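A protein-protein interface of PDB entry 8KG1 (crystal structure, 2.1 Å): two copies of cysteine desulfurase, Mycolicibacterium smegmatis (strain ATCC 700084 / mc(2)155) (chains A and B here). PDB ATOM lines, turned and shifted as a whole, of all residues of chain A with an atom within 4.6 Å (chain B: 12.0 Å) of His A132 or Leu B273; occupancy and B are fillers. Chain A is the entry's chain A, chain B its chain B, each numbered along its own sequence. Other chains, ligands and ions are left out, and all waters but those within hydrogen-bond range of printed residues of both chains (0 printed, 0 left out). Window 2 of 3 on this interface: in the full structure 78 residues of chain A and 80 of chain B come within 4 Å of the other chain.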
ATOM      1  N   ILE A 130     -26.865 -17.783 -20.283  1.00  0.00           N
ATOM      2  CA  ILE A 130     -27.354 -16.531 -19.713  1.00  0.00           C
ATOM      3  C   ILE A 130     -26.212 -15.520 -19.760  1.00  0.00           C
ATOM      4  O   ILE A 130     -25.056 -15.864 -19.999  1.00  0.00           O
ATOM      5  CB  ILE A 130     -27.875 -16.692 -18.269  1.00  0.00           C
ATOM      6  CG1 ILE A 130     -26.736 -17.102 -17.333  1.00  0.00           C
ATOM      7  CG2 ILE A 130     -29.003 -17.702 -18.203  1.00  0.00           C
ATOM      8  CD1 ILE A 130     -27.078 -16.952 -15.842  1.00  0.00           C
ATOM      9  N   THR A 131     -26.545 -14.261 -19.540  1.00  0.00           N
ATOM     10  CA  THR A 131     -25.510 -13.242 -19.494  1.00  0.00           C
ATOM     11  C   THR A 131     -25.125 -12.981 -18.046  1.00  0.00           C
ATOM     12  O   THR A 131     -25.872 -13.283 -17.115  1.00  0.00           O
ATOM     13  CB  THR A 131     -25.963 -11.943 -20.177  1.00  0.00           C
ATOM     14  OG1 THR A 131     -26.860 -11.242 -19.313  1.00  0.00           O
ATOM     15  CG2 THR A 131     -26.673 -12.235 -21.493  1.00  0.00           C
ATOM     16  N   HIS A 132     -23.922 -12.441 -17.863  1.00  0.00           N
ATOM     17  CA  HIS A 132     -23.459 -12.098 -16.528  1.00  0.00           C
ATOM     18  C   HIS A 132     -24.296 -10.989 -15.888  1.00  0.00           C
ATOM     19  O   HIS A 132     -24.188 -10.775 -14.673  1.00  0.00           O
ATOM     20  CB  HIS A 132     -21.985 -11.686 -16.604  1.00  0.00           C
ATOM     21  CG  HIS A 132     -21.190 -12.074 -15.401  1.00  0.00           C
ATOM     22  ND1 HIS A 132     -19.819 -12.223 -15.431  1.00  0.00           N
ATOM     23  CD2 HIS A 132     -21.572 -12.351 -14.132  1.00  0.00           C
ATOM     24  CE1 HIS A 132     -19.391 -12.574 -14.231  1.00  0.00           C
ATOM     25  NE2 HIS A 132     -20.434 -12.654 -13.423  1.00  0.00           N
ATOM     26  N   LEU A 133     -25.141 -10.305 -16.671  1.00  0.00           N
ATOM     27  CA  LEU A 133     -25.939  -9.154 -16.236  1.00  0.00           C
ATOM     28  C   LEU A 133     -27.236  -9.528 -15.528  1.00  0.00           C
ATOM     29  O   LEU A 133     -27.977  -8.623 -15.125  1.00  0.00           O
ATOM     30  CB  LEU A 133     -26.276  -8.289 -17.454  1.00  0.00           C
ATOM     31  CG  LEU A 133     -25.054  -7.645 -18.097  1.00  0.00           C
ATOM     32  CD1 LEU A 133     -25.420  -7.072 -19.450  1.00  0.00           C
ATOM     33  CD2 LEU A 133     -24.562  -6.552 -17.184  1.00  0.00           C
ATOM     34  N   GLU A 134     -27.528 -10.818 -15.371  1.00  0.00           N
ATOM     35  CA  GLU A 134     -28.861 -11.255 -14.970  1.00  0.00           C
ATOM     36  C   GLU A 134     -29.192 -10.896 -13.524  1.00  0.00           C
ATOM     37  O   GLU A 134     -28.351 -10.985 -12.626  1.00  0.00           O
ATOM     38  CB  GLU A 134     -28.992 -12.772 -15.151  1.00  0.00           C
ATOM     39  CG  GLU A 134     -28.903 -13.298 -16.594  1.00  0.00           C
ATOM     40  CD  GLU A 134     -29.605 -12.424 -17.641  1.00  0.00           C
ATOM     41  OE1 GLU A 134     -30.798 -12.084 -17.439  1.00  0.00           O
ATOM     42  OE2 GLU A 134     -28.959 -12.075 -18.670  1.00  0.00           O
ATOM     43  N   GLN A 143     -30.444 -22.529 -12.473  1.00  0.00           N
ATOM     44  CA  GLN A 143     -29.635 -23.402 -11.614  1.00  0.00           C
ATOM     45  C   GLN A 143     -30.446 -24.589 -11.104  1.00  0.00           C
ATOM     46  O   GLN A 143     -29.954 -25.730 -11.085  1.00  0.00           O
ATOM     47  CB  GLN A 143     -29.056 -22.610 -10.438  1.00  0.00           C
ATOM     48  CG  GLN A 143     -27.995 -21.572 -10.825  1.00  0.00           C
ATOM     49  CD  GLN A 143     -27.587 -20.672  -9.659  1.00  0.00           C
ATOM     50  OE1 GLN A 143     -28.395 -20.356  -8.777  1.00  0.00           O
ATOM     51  NE2 GLN A 143     -26.333 -20.255  -9.655  1.00  0.00           N
ATOM     52  N   VAL A 155     -22.328 -18.743 -18.924  1.00  0.00           N
ATOM     53  CA  VAL A 155     -22.536 -17.338 -18.577  1.00  0.00           C
ATOM     54  C   VAL A 155     -21.730 -16.477 -19.549  1.00  0.00           C
ATOM     55  O   VAL A 155     -20.495 -16.500 -19.530  1.00  0.00           O
ATOM     56  CB  VAL A 155     -22.134 -17.047 -17.126  1.00  0.00           C
ATOM     57  CG1 VAL A 155     -22.417 -15.582 -16.772  1.00  0.00           C
ATOM     58  CG2 VAL A 155     -22.862 -18.003 -16.162  1.00  0.00           C
ATOM     59  N   ALA A 156     -22.423 -15.713 -20.385  1.00  0.00           N
ATOM     60  CA  ALA A 156     -21.756 -14.821 -21.336  1.00  0.00           C
ATOM     61  C   ALA A 156     -21.134 -13.637 -20.602  1.00  0.00           C
ATOM     62  O   ALA A 156     -21.792 -13.034 -19.749  1.00  0.00           O
ATOM     63  CB  ALA A 156     -22.755 -14.324 -22.376  1.00  0.00           C
ATOM     64  N   PRO A 157     -19.885 -13.272 -20.900  1.00  0.00           N
ATOM     65  CA  PRO A 157     -19.183 -12.256 -20.102  1.00  0.00           C
ATOM     66  C   PRO A 157     -19.417 -10.821 -20.564  1.00  0.00           C
ATOM     67  O   PRO A 157     -19.909 -10.556 -21.662  1.00  0.00           O
ATOM     68  CB  PRO A 157     -17.706 -12.645 -20.279  1.00  0.00           C
ATOM     69  CG  PRO A 157     -17.650 -13.308 -21.614  1.00  0.00           C
ATOM     70  CD  PRO A 157     -18.987 -13.967 -21.845  1.00  0.00           C
ATOM     71  N   VAL A 158     -19.056  -9.887 -19.681  1.00  0.00           N
ATOM     72  CA  VAL A 158     -19.134  -8.456 -19.947  1.00  0.00           C
ATOM     73  C   VAL A 158     -17.733  -7.874 -19.798  1.00  0.00           C
ATOM     74  O   VAL A 158     -16.876  -8.444 -19.116  1.00  0.00           O
ATOM     75  CB  VAL A 158     -20.113  -7.723 -18.995  1.00  0.00           C
ATOM     76  CG1 VAL A 158     -21.559  -8.181 -19.214  1.00  0.00           C
ATOM     77  CG2 VAL A 158     -19.693  -7.933 -17.537  1.00  0.00           C
ATOM     78  N   PRO A 379     -23.975 -11.643  -8.876  1.00  0.00           N
ATOM     79  CA  PRO A 379     -22.858 -12.016  -9.762  1.00  0.00           C
ATOM     80  C   PRO A 379     -22.290 -10.846 -10.546  1.00  0.00           C
ATOM     81  O   PRO A 379     -21.062 -10.713 -10.628  1.00  0.00           O
ATOM     82  CB  PRO A 379     -23.480 -13.087 -10.668  1.00  0.00           C
ATOM     83  CG  PRO A 379     -24.481 -13.751  -9.767  1.00  0.00           C
ATOM     84  CD  PRO A 379     -25.118 -12.553  -9.066  1.00  0.00           C
ATOM     85  N   ILE A 380     -23.138  -9.972 -11.099  1.00  0.00           N
ATOM     86  CA  ILE A 380     -22.612  -8.831 -11.847  1.00  0.00           C
ATOM     87  C   ILE A 380     -21.847  -7.888 -10.925  1.00  0.00           C
ATOM     88  O   ILE A 380     -20.816  -7.327 -11.315  1.00  0.00           O
ATOM     89  CB  ILE A 380     -23.732  -8.104 -12.619  1.00  0.00           C
ATOM     90  CG1 ILE A 380     -23.120  -7.064 -13.571  1.00  0.00           C
ATOM     91  CG2 ILE A 380     -24.712  -7.413 -11.681  1.00  0.00           C
ATOM     92  CD1 ILE A 380     -22.095  -7.615 -14.552  1.00  0.00           C
ATOM     93  N   ARG A 383     -18.510  -9.401 -10.323  1.00  0.00           N
ATOM     94  CA  ARG A 383     -17.701  -9.198 -11.520  1.00  0.00           C
ATOM     95  C   ARG A 383     -17.095  -7.802 -11.537  1.00  0.00           C
ATOM     96  O   ARG A 383     -15.975  -7.617 -12.031  1.00  0.00           O
ATOM     97  CB  ARG A 383     -18.550  -9.450 -12.774  1.00  0.00           C
ATOM     98  CG  ARG A 383     -18.025  -8.825 -14.077  1.00  0.00           C
ATOM     99  CD  ARG A 383     -16.751  -9.521 -14.562  1.00  0.00           C
ATOM    100  NE  ARG A 383     -16.334  -9.028 -15.871  1.00  0.00           N
ATOM    101  CZ  ARG A 383     -15.533  -7.986 -16.050  1.00  0.00           C
ATOM    102  NH1 ARG A 383     -15.054  -7.300 -15.023  1.00  0.00           N
ATOM    103  NH2 ARG A 383     -15.212  -7.617 -17.288  1.00  0.00           N
ATOM    104  N   ILE B 268     -33.765 -16.206  -1.998  1.00  0.00           N
ATOM    105  CA  ILE B 268     -32.355 -16.566  -1.856  1.00  0.00           C
ATOM    106  C   ILE B 268     -31.750 -15.806  -0.680  1.00  0.00           C
ATOM    107  O   ILE B 268     -32.200 -14.720  -0.309  1.00  0.00           O
ATOM    108  CB  ILE B 268     -31.547 -16.303  -3.148  1.00  0.00           C
ATOM    109  CG1 ILE B 268     -31.671 -14.839  -3.591  1.00  0.00           C
ATOM    110  CG2 ILE B 268     -31.961 -17.247  -4.254  1.00  0.00           C
ATOM    111  CD1 ILE B 268     -30.536 -13.951  -3.064  1.00  0.00           C
ATOM    112  N   ALA B 269     -30.702 -16.383  -0.100  1.00  0.00           N
ATOM    113  CA  ALA B 269     -29.813 -15.684   0.817  1.00  0.00           C
ATOM    114  C   ALA B 269     -28.521 -15.239   0.149  1.00  0.00           C
ATOM    115  O   ALA B 269     -27.979 -14.187   0.502  1.00  0.00           O
ATOM    116  CB  ALA B 269     -29.481 -16.583   2.014  1.00  0.00           C
ATOM    117  N   ASP B 270     -28.033 -16.003  -0.828  1.00  0.00           N
ATOM    118  CA  ASP B 270     -26.795 -15.695  -1.532  1.00  0.00           C
ATOM    119  C   ASP B 270     -26.803 -16.379  -2.891  1.00  0.00           C
ATOM    120  O   ASP B 270     -27.197 -17.544  -3.002  1.00  0.00           O
ATOM    121  CB  ASP B 270     -25.571 -16.152  -0.731  1.00  0.00           C
ATOM    122  CG  ASP B 270     -24.275 -15.698  -1.358  1.00  0.00           C
ATOM    123  OD1 ASP B 270     -23.930 -14.509  -1.196  1.00  0.00           O
ATOM    124  OD2 ASP B 270     -23.597 -16.530  -2.002  1.00  0.00           O
ATOM    125  N   VAL B 271     -26.361 -15.654  -3.916  1.00  0.00           N
ATOM    126  CA  VAL B 271     -26.269 -16.185  -5.270  1.00  0.00           C
ATOM    127  C   VAL B 271     -24.855 -15.964  -5.788  1.00  0.00           C
ATOM    128  O   VAL B 271     -24.337 -14.840  -5.742  1.00  0.00           O
ATOM    129  CB  VAL B 271     -27.295 -15.530  -6.216  1.00  0.00           C
ATOM    130  CG1 VAL B 271     -27.091 -16.008  -7.662  1.00  0.00           C
ATOM    131  CG2 VAL B 271     -28.712 -15.831  -5.749  1.00  0.00           C
ATOM    132  N   THR B 272     -24.225 -17.039  -6.248  1.00  0.00           N
ATOM    133  CA  THR B 272     -23.085 -16.978  -7.149  1.00  0.00           C
ATOM    134  C   THR B 272     -23.466 -17.719  -8.422  1.00  0.00           C
ATOM    135  O   THR B 272     -24.485 -18.405  -8.471  1.00  0.00           O
ATOM    136  CB  THR B 272     -21.828 -17.591  -6.521  1.00  0.00           C
ATOM    137  OG1 THR B 272     -21.934 -19.017  -6.548  1.00  0.00           O
ATOM    138  CG2 THR B 272     -21.643 -17.107  -5.084  1.00  0.00           C
ATOM    139  N   LEU B 273     -22.651 -17.570  -9.471  1.00  0.00           N
ATOM    140  CA  LEU B 273     -22.933 -18.312 -10.695  1.00  0.00           C
ATOM    141  C   LEU B 273     -22.933 -19.814 -10.442  1.00  0.00           C
ATOM    142  O   LEU B 273     -23.633 -20.563 -11.134  1.00  0.00           O
ATOM    143  CB  LEU B 273     -21.918 -17.958 -11.783  1.00  0.00           C
ATOM    144  CG  LEU B 273     -21.976 -16.492 -12.229  1.00  0.00           C
ATOM    145  CD1 LEU B 273     -21.010 -16.230 -13.384  1.00  0.00           C
ATOM    146  CD2 LEU B 273     -23.396 -16.110 -12.609  1.00  0.00           C
ATOM    147  N   GLU B 274     -22.183 -20.266  -9.436  1.00  0.00           N
ATOM    148  CA  GLU B 274     -22.065 -21.693  -9.172  1.00  0.00           C
ATOM    149  C   GLU B 274     -23.291 -22.243  -8.440  1.00  0.00           C
ATOM    150  O   GLU B 274     -23.810 -23.300  -8.811  1.00  0.00           O
ATOM    151  CB  GLU B 274     -20.778 -21.979  -8.386  1.00  0.00           C
ATOM    152  CG  GLU B 274     -20.346 -23.445  -8.467  1.00  0.00           C
ATOM    153  CD  GLU B 274     -19.545 -23.914  -7.259  1.00  0.00           C
ATOM    154  OE1 GLU B 274     -19.806 -23.437  -6.130  1.00  0.00           O
ATOM    155  OE2 GLU B 274     -18.665 -24.783  -7.441  1.00  0.00           O
ATOM    156  N   ARG B 275     -23.781 -21.543  -7.413  1.00  0.00           N
ATOM    157  CA  ARG B 275     -24.866 -22.084  -6.601  1.00  0.00           C
ATOM    158  C   ARG B 275     -25.556 -20.955  -5.853  1.00  0.00           C
ATOM    159  O   ARG B 275     -24.992 -19.877  -5.668  1.00  0.00           O
ATOM    160  CB  ARG B 275     -24.356 -23.125  -5.601  1.00  0.00           C
ATOM    161  CG  ARG B 275     -23.260 -22.596  -4.682  1.00  0.00           C
ATOM    162  CD  ARG B 275     -23.854 -22.181  -3.344  1.00  0.00           C
ATOM    163  NE  ARG B 275     -22.976 -21.330  -2.548  1.00  0.00           N
ATOM    164  CZ  ARG B 275     -23.125 -20.021  -2.389  1.00  0.00           C
ATOM    165  NH1 ARG B 275     -24.014 -19.329  -3.093  1.00  0.00           N
ATOM    166  NH2 ARG B 275     -22.357 -19.387  -1.509  1.00  0.00           N
ATOM    167  N   SER B 276     -26.779 -21.224  -5.402  1.00  0.00           N
ATOM    168  CA  SER B 276     -27.535 -20.289  -4.579  1.00  0.00           C
ATOM    169  C   SER B 276     -27.941 -20.956  -3.277  1.00  0.00           C
ATOM    170  O   SER B 276     -28.331 -22.126  -3.271  1.00  0.00           O
ATOM    171  CB  SER B 276     -28.784 -19.789  -5.307  1.00  0.00           C
ATOM    172  OG  SER B 276     -28.433 -19.142  -6.516  1.00  0.00           O
ATOM    173  N   LEU B 277     -27.836 -20.214  -2.179  1.00  0.00           N
ATOM    174  CA  LEU B 277     -28.307 -20.654  -0.871  1.00  0.00           C
ATOM    175  C   LEU B 277     -29.654 -20.006  -0.594  1.00  0.00           C
ATOM    176  O   LEU B 277     -29.903 -18.883  -1.013  1.00  0.00           O
ATOM    177  CB  LEU B 277     -27.311 -20.277   0.234  1.00  0.00           C
ATOM    178  CG  LEU B 277     -25.851 -20.682   0.017  1.00  0.00           C
ATOM    179  CD1 LEU B 277     -24.971 -20.282   1.212  1.00  0.00           C
ATOM    180  CD2 LEU B 277     -25.780 -22.172  -0.220  1.00  0.00           C
ATOM    181  N   TYR B 278     -30.521 -20.704   0.127  1.00  0.00           N
ATOM    182  CA  TYR B 278     -31.901 -20.263   0.277  1.00  0.00           C
ATOM    183  C   TYR B 278     -32.160 -19.755   1.686  1.00  0.00           C
ATOM    184  O   TYR B 278     -31.499 -20.161   2.650  1.00  0.00           O
ATOM    185  CB  TYR B 278     -32.871 -21.405  -0.079  1.00  0.00           C
ATOM    186  CG  TYR B 278     -32.637 -21.858  -1.501  1.00  0.00           C
ATOM    187  CD1 TYR B 278     -32.672 -20.937  -2.544  1.00  0.00           C
ATOM    188  CD2 TYR B 278     -32.274 -23.169  -1.793  1.00  0.00           C
ATOM    189  CE1 TYR B 278     -32.415 -21.319  -3.859  1.00  0.00           C
ATOM    190  CE2 TYR B 278     -32.007 -23.566  -3.116  1.00  0.00           C
ATOM    191  CZ  TYR B 278     -32.083 -22.631  -4.142  1.00  0.00           C
ATOM    192  OH  TYR B 278     -31.822 -22.992  -5.450  1.00  0.00           O
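Among the printed residues, pairs that only touch across the chains: His A132 with Leu B273 (3.6 Å), Gln A143 with Glu B274 (3.8 Å), Gln A143 with Arg B275 (3.6 Å), Val A155 with Leu B273 (3.7 Å) and Pro A379 with Leu B273 (3.6 Å).
The backbone carbonyl oxygen (O) of Ala A156 sits at hydrogen-bond distance from the backbone NH (N) of His A132 (2.9 Å). A ring nitrogen (NE2) of His A132 is in hydrogen-bond range of the backbone carbonyl oxygen of Pro A379. OD2 of Asp B270 lies within salt-bridge range of NH1 of Arg B275 (3.0 Å). OG1 of Thr B272 sits close to N of Glu B274 (3.2 Å). The side-chain hydroxyl (OG1) of Thr B272 is in hydrogen-bond range of the backbone NH (N) of Arg B275, at 3.2 Å.
No residue of chain B comes within 4 Å of Ile A130. His A132 touches just one residue of chain B: Leu B273 (3.6 Å). No residue of chain B comes within 4 Å of Leu A133. No residue of chain B comes within 4 Å of Glu A134. Of chain B, only Leu B273 (3.7 Å) comes within 4 Å of Val A155. No residue of chain B comes within 4 Å of Pro A157. No residue of chain B comes within 4 Å of Val A158. Pro A379 touches just one residue of chain B: Leu B273. No residue of chain B comes within 4 Å of Arg A383. Of the printed residues of chain A, Thr B272 touches Gln A143 (2.9 Å). Leu B273 touches just these residues of chain A: His A132, Gln A143, Val A155 and Pro A379. Of the printed residues of chain A, Ser B276 touches Gln A143. The nearest residue of chain B that does not touch His A132 is Thr B272 (7.7 Å). The nearest printed residue of chain A that does not touch Leu B273 is Ile A130 (5.0 Å). The nearest printed residue of chain A that does not touch Arg B275 is Pro A379 (7.4 Å).
No position is printed for both chains. Of the 8 pairs that touch across the chains among the printed residues, none has its exchanged pair printed and touching as well.
The side-chain amide nitrogen (NE2) of Gln A143 is in hydrogen-bond range of the backbone carbonyl oxygen (O) of Thr B272 (2.9 Å). The side-chain amide nitrogen of Gln A143 lies within hydrogen-bond range of the backbone carbonyl oxygen of Leu B273 (3.1 Å). The side-chain amide oxygen (OE1) of Gln A143 is in hydrogen-bond range of the side-chain hydroxyl (OG) of Ser B276 (2.6 Å).
Of the 13 printed residues of chain A, 4 touch a printed residue of chain B. Hydrophobic or aromatic side chains of chain A that line the printed part of chain B: His A132, Val A155 and Pro A379. Printed residues of chain B that touch a printed residue of chain A: Thr B272, Leu B273, Glu B274, Arg B275 and Ser B276. Among the printed residues, no Asp or Glu carboxylate lies within 4 Å of a Lys or Arg side-chain nitrogen of the other chain.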
